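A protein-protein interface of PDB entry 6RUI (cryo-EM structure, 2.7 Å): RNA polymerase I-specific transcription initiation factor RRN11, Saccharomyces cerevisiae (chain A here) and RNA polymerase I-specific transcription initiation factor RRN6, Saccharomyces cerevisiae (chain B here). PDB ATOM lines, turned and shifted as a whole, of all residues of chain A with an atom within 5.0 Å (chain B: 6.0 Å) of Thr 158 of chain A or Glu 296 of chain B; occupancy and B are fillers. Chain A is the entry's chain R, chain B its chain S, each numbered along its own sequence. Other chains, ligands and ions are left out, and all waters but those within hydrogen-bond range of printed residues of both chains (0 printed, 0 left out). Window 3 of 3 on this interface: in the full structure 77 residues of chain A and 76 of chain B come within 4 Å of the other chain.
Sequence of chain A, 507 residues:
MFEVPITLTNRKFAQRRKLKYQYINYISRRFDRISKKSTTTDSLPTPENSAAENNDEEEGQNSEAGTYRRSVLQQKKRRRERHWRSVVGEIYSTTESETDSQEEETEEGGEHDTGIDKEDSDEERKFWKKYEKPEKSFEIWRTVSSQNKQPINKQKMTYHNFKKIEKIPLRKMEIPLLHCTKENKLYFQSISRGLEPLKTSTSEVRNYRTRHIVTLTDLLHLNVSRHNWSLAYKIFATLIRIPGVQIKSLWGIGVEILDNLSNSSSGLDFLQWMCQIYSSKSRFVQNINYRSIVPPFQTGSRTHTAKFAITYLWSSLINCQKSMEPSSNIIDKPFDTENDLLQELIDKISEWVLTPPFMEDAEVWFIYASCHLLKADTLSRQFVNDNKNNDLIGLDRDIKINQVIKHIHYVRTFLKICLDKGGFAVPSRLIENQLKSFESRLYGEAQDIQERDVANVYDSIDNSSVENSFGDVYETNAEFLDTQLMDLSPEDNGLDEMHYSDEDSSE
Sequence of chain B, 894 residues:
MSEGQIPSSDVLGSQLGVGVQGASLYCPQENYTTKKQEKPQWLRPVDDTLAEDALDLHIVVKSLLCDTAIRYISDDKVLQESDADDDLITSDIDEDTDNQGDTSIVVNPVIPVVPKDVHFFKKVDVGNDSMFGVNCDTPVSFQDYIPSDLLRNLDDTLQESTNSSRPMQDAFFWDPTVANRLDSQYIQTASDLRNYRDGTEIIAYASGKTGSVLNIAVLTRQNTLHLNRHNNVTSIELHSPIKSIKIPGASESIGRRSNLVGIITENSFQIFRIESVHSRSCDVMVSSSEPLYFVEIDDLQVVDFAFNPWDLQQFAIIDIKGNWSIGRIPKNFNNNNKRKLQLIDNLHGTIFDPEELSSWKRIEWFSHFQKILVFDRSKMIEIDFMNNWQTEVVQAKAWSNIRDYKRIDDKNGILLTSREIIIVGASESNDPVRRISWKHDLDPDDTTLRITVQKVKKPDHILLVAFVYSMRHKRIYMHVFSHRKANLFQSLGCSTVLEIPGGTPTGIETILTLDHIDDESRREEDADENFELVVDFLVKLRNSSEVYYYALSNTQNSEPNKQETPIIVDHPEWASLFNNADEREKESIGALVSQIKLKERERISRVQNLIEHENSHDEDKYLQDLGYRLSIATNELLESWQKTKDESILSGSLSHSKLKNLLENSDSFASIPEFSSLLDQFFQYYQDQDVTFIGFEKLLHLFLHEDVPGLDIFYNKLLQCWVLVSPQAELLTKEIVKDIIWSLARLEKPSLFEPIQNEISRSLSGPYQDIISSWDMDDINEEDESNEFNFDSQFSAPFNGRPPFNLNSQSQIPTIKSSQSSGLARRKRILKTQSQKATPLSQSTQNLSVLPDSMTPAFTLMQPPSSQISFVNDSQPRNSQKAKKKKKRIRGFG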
ATOM      1  N   LYS A 156     -15.395 -13.163  -3.052  1.00  0.00           N
ATOM      2  CA  LYS A 156     -16.111 -11.901  -3.055  1.00  0.00           C
ATOM      3  C   LYS A 156     -15.943 -11.177  -1.726  1.00  0.00           C
ATOM      4  O   LYS A 156     -15.331 -11.683  -0.783  1.00  0.00           O
ATOM      5  CB  LYS A 156     -17.597 -12.116  -3.342  1.00  0.00           C
ATOM      6  CG  LYS A 156     -18.311 -12.932  -2.286  1.00  0.00           C
ATOM      7  CD  LYS A 156     -19.770 -13.122  -2.646  1.00  0.00           C
ATOM      8  CE  LYS A 156     -20.471 -13.988  -1.630  1.00  0.00           C
ATOM      9  NZ  LYS A 156     -19.957 -15.380  -1.687  1.00  0.00           N
ATOM     10  N   MET A 157     -16.504  -9.973  -1.674  1.00  0.00           N
ATOM     11  CA  MET A 157     -16.404  -9.088  -0.526  1.00  0.00           C
ATOM     12  C   MET A 157     -17.371  -9.502   0.579  1.00  0.00           C
ATOM     13  O   MET A 157     -18.269 -10.326   0.384  1.00  0.00           O
ATOM     14  CB  MET A 157     -16.701  -7.648  -0.948  1.00  0.00           C
ATOM     15  CG  MET A 157     -15.649  -7.040  -1.831  1.00  0.00           C
ATOM     16  SD  MET A 157     -14.106  -6.854  -0.934  1.00  0.00           S
ATOM     17  CE  MET A 157     -14.571  -5.558   0.205  1.00  0.00           C
ATOM     18  N   THR A 158     -17.175  -8.911   1.758  1.00  0.00           N
ATOM     19  CA  THR A 158     -18.192  -8.911   2.800  1.00  0.00           C
ATOM     20  C   THR A 158     -18.099  -7.606   3.580  1.00  0.00           C
ATOM     21  O   THR A 158     -17.163  -6.817   3.415  1.00  0.00           O
ATOM     22  CB  THR A 158     -18.062 -10.113   3.740  1.00  0.00           C
ATOM     23  OG1 THR A 158     -19.224 -10.187   4.577  1.00  0.00           O
ATOM     24  CG2 THR A 158     -16.852  -9.964   4.626  1.00  0.00           C
ATOM     25  N   TYR A 159     -19.095  -7.391   4.439  1.00  0.00           N
ATOM     26  CA  TYR A 159     -19.145  -6.195   5.271  1.00  0.00           C
ATOM     27  C   TYR A 159     -18.049  -6.187   6.322  1.00  0.00           C
ATOM     28  O   TYR A 159     -17.605  -5.114   6.741  1.00  0.00           O
ATOM     29  CB  TYR A 159     -20.508  -6.107   5.945  1.00  0.00           C
ATOM     30  CG  TYR A 159     -20.700  -4.900   6.825  1.00  0.00           C
ATOM     31  CD1 TYR A 159     -20.912  -3.639   6.274  1.00  0.00           C
ATOM     32  CD2 TYR A 159     -20.685  -5.019   8.208  1.00  0.00           C
ATOM     33  CE1 TYR A 159     -21.095  -2.527   7.082  1.00  0.00           C
ATOM     34  CE2 TYR A 159     -20.869  -3.915   9.021  1.00  0.00           C
ATOM     35  CZ  TYR A 159     -21.074  -2.674   8.453  1.00  0.00           C
ATOM     36  OH  TYR A 159     -21.256  -1.583   9.265  1.00  0.00           O
ATOM     37  N   HIS A 160     -17.609  -7.365   6.767  1.00  0.00           N
ATOM     38  CA  HIS A 160     -16.554  -7.424   7.769  1.00  0.00           C
ATOM     39  C   HIS A 160     -15.202  -7.056   7.181  1.00  0.00           C
ATOM     40  O   HIS A 160     -14.399  -6.399   7.849  1.00  0.00           O
ATOM     41  CB  HIS A 160     -16.510  -8.816   8.390  1.00  0.00           C
ATOM     42  CG  HIS A 160     -17.736  -9.154   9.179  1.00  0.00           C
ATOM     43  ND1 HIS A 160     -18.863  -9.699   8.603  1.00  0.00           N
ATOM     44  CD2 HIS A 160     -18.012  -9.022  10.497  1.00  0.00           C
ATOM     45  CE1 HIS A 160     -19.781  -9.889   9.533  1.00  0.00           C
ATOM     46  NE2 HIS A 160     -19.290  -9.486  10.691  1.00  0.00           N
ATOM     47  N   ASN A 161     -14.941  -7.446   5.937  1.00  0.00           N
ATOM     48  CA  ASN A 161     -13.705  -7.061   5.279  1.00  0.00           C
ATOM     49  C   ASN A 161     -13.734  -5.645   4.738  1.00  0.00           C
ATOM     50  O   ASN A 161     -12.673  -5.030   4.615  1.00  0.00           O
ATOM     51  CB  ASN A 161     -13.369  -8.009   4.124  1.00  0.00           C
ATOM     52  CG  ASN A 161     -13.017  -9.403   4.593  1.00  0.00           C
ATOM     53  OD1 ASN A 161     -13.653 -10.378   4.208  1.00  0.00           O
ATOM     54  ND2 ASN A 161     -12.001  -9.502   5.437  1.00  0.00           N
ATOM     55  N   PHE A 162     -14.911  -5.110   4.409  1.00  0.00           N
ATOM     56  CA  PHE A 162     -14.953  -3.767   3.839  1.00  0.00           C
ATOM     57  C   PHE A 162     -14.758  -2.687   4.894  1.00  0.00           C
ATOM     58  O   PHE A 162     -14.094  -1.678   4.632  1.00  0.00           O
ATOM     59  CB  PHE A 162     -16.261  -3.536   3.086  1.00  0.00           C
ATOM     60  CG  PHE A 162     -16.430  -2.122   2.606  1.00  0.00           C
ATOM     61  CD1 PHE A 162     -15.537  -1.579   1.695  1.00  0.00           C
ATOM     62  CD2 PHE A 162     -17.500  -1.350   3.035  1.00  0.00           C
ATOM     63  CE1 PHE A 162     -15.689  -0.276   1.245  1.00  0.00           C
ATOM     64  CE2 PHE A 162     -17.663  -0.047   2.582  1.00  0.00           C
ATOM     65  CZ  PHE A 162     -16.757   0.487   1.683  1.00  0.00           C
ATOM     66  N   PHE B 294     -30.508 -11.216   5.427  1.00  0.00           N
ATOM     67  CA  PHE B 294     -29.110 -11.027   5.069  1.00  0.00           C
ATOM     68  C   PHE B 294     -28.223 -11.934   5.909  1.00  0.00           C
ATOM     69  O   PHE B 294     -28.225 -11.855   7.142  1.00  0.00           O
ATOM     70  CB  PHE B 294     -28.724  -9.564   5.230  1.00  0.00           C
ATOM     71  CG  PHE B 294     -29.339  -8.680   4.203  1.00  0.00           C
ATOM     72  CD1 PHE B 294     -28.750  -8.534   2.958  1.00  0.00           C
ATOM     73  CD2 PHE B 294     -30.527  -8.025   4.462  1.00  0.00           C
ATOM     74  CE1 PHE B 294     -29.322  -7.722   1.999  1.00  0.00           C
ATOM     75  CE2 PHE B 294     -31.102  -7.221   3.506  1.00  0.00           C
ATOM     76  CZ  PHE B 294     -30.499  -7.066   2.278  1.00  0.00           C
ATOM     77  N   VAL B 295     -27.481 -12.809   5.234  1.00  0.00           N
ATOM     78  CA  VAL B 295     -26.378 -13.513   5.872  1.00  0.00           C
ATOM     79  C   VAL B 295     -25.155 -12.606   5.949  1.00  0.00           C
ATOM     80  O   VAL B 295     -24.466 -12.549   6.973  1.00  0.00           O
ATOM     81  CB  VAL B 295     -26.085 -14.819   5.108  1.00  0.00           C
ATOM     82  CG1 VAL B 295     -24.985 -15.618   5.794  1.00  0.00           C
ATOM     83  CG2 VAL B 295     -27.355 -15.646   4.968  1.00  0.00           C
ATOM     84  N   GLU B 296     -24.876 -11.875   4.866  1.00  0.00           N
ATOM     85  CA  GLU B 296     -23.888 -10.801   4.871  1.00  0.00           C
ATOM     86  C   GLU B 296     -24.599  -9.451   4.927  1.00  0.00           C
ATOM     87  O   GLU B 296     -25.630  -9.248   4.277  1.00  0.00           O
ATOM     88  CB  GLU B 296     -22.964 -10.896   3.650  1.00  0.00           C
ATOM     89  CG  GLU B 296     -23.590 -10.647   2.274  1.00  0.00           C
ATOM     90  CD  GLU B 296     -24.223 -11.890   1.662  1.00  0.00           C
ATOM     91  OE1 GLU B 296     -24.516 -12.858   2.396  1.00  0.00           O
ATOM     92  OE2 GLU B 296     -24.413 -11.905   0.431  1.00  0.00           O
ATOM     93  N   ILE B 297     -24.075  -8.545   5.745  1.00  0.00           N
ATOM     94  CA  ILE B 297     -24.809  -7.323   6.101  1.00  0.00           C
ATOM     95  C   ILE B 297     -24.376  -6.257   5.101  1.00  0.00           C
ATOM     96  O   ILE B 297     -23.593  -5.352   5.393  1.00  0.00           O
ATOM     97  CB  ILE B 297     -24.557  -6.926   7.559  1.00  0.00           C
ATOM     98  CG1 ILE B 297     -24.835  -8.134   8.459  1.00  0.00           C
ATOM     99  CG2 ILE B 297     -25.465  -5.769   7.989  1.00  0.00           C
ATOM    100  CD1 ILE B 297     -24.333  -7.991   9.871  1.00  0.00           C
ATOM    101  N   ASP B 298     -24.960  -6.327   3.901  1.00  0.00           N
ATOM    102  CA  ASP B 298     -24.633  -5.423   2.798  1.00  0.00           C
ATOM    103  C   ASP B 298     -25.870  -5.242   1.932  1.00  0.00           C
ATOM    104  O   ASP B 298     -26.467  -6.226   1.486  1.00  0.00           O
ATOM    105  CB  ASP B 298     -23.464  -5.954   1.956  1.00  0.00           C
ATOM    106  CG  ASP B 298     -22.103  -5.706   2.592  1.00  0.00           C
ATOM    107  OD1 ASP B 298     -21.920  -4.660   3.246  1.00  0.00           O
ATOM    108  OD2 ASP B 298     -21.207  -6.557   2.431  1.00  0.00           O
ATOM    109  N   ASP B 299     -26.237  -3.987   1.684  1.00  0.00           N
ATOM    110  CA  ASP B 299     -27.543  -3.652   1.123  1.00  0.00           C
ATOM    111  C   ASP B 299     -27.528  -3.883  -0.387  1.00  0.00           C
ATOM    112  O   ASP B 299     -26.834  -3.176  -1.125  1.00  0.00           O
ATOM    113  CB  ASP B 299     -27.891  -2.207   1.466  1.00  0.00           C
ATOM    114  CG  ASP B 299     -29.350  -1.871   1.220  1.00  0.00           C
ATOM    115  OD1 ASP B 299     -30.119  -2.747   0.781  1.00  0.00           O
ATOM    116  OD2 ASP B 299     -29.736  -0.710   1.470  1.00  0.00           O
ATOM    117  N   ILE B 320     -25.435  -6.917  -4.982  1.00  0.00           N
ATOM    118  CA  ILE B 320     -25.124  -6.324  -3.688  1.00  0.00           C
ATOM    119  C   ILE B 320     -24.105  -5.220  -3.962  1.00  0.00           C
ATOM    120  O   ILE B 320     -23.595  -5.111  -5.083  1.00  0.00           O
ATOM    121  CB  ILE B 320     -24.600  -7.404  -2.723  1.00  0.00           C
ATOM    122  CG1 ILE B 320     -25.445  -8.665  -2.846  1.00  0.00           C
ATOM    123  CG2 ILE B 320     -24.783  -7.010  -1.278  1.00  0.00           C
ATOM    124  CD1 ILE B 320     -24.836  -9.874  -2.166  1.00  0.00           C
ATOM    125  N   ASN B 323     -20.692  -7.041  -5.148  1.00  0.00           N
ATOM    126  CA  ASN B 323     -20.652  -8.430  -5.590  1.00  0.00           C
ATOM    127  C   ASN B 323     -22.054  -8.911  -5.927  1.00  0.00           C
ATOM    128  O   ASN B 323     -23.046  -8.360  -5.447  1.00  0.00           O
ATOM    129  CB  ASN B 323     -19.990  -9.330  -4.535  1.00  0.00           C
ATOM    130  CG  ASN B 323     -20.515  -9.090  -3.138  1.00  0.00           C
ATOM    131  OD1 ASN B 323     -21.478  -8.358  -2.933  1.00  0.00           O
ATOM    132  ND2 ASN B 323     -19.846  -9.680  -2.160  1.00  0.00           N
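The backbone NH of Tyr 159 of chain A sits at hydrogen-bond distance from the side-chain carboxylate of Asp 298 of chain B, at 3.0 Å.
The side-chain amide nitrogen (ND2) of Asn 323 of chain B is in hydrogen-bond range of the backbone carbonyl oxygen (O) of Met 157 of chain A, at 3.1 Å.
Among the printed residues, merely in contact across the chains: Tyr 159 of chain A with Ile 297 of chain B (3.2 Å), Thr 158 of chain A with Asp 298 of chain B (3.5 Å), Lys 156 of chain A with Asn 323 of chain B (3.5 Å) and Thr 158 of chain A with Glu 296 of chain B (3.9 Å).
Of the printed residues of chain B, Thr 158 of chain A touches Glu 296 (3.9 Å) and Asp 298 (3.5 Å).
Of the printed residues of chain B, Tyr 159 of chain A touches Ile 297 (3.2 Å) and Asp 298 (3.0 Å).
Val 295 of chain B touches none of the printed residues of chain A.
Printed residues of chain A within 4 Å of Glu 296 of chain B: Thr 158 (3.9 Å).
Printed residues of chain A within 4 Å of Asp 298 of chain B: Thr 158 (3.5 Å) and Tyr 159 (3.0 Å).
Ile 320 of chain B touches none of the printed residues of chain A.
Of the printed residues of chain A, Asn 323 of chain B touches Lys 156 and Met 157.
The nearest printed residue of chain B that does not touch Met 157 of chain A is Asp 298 of chain B (5.2 Å).
Of the 8 printed residues of chain B, 4 touch a printed residue of chain A.
Among the printed residues, 6 pairs touch across the chains.
Among the printed residues, no Asp or Glu carboxylate lies within 4 Å of a Lys or Arg side-chain nitrogen of the other chain.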
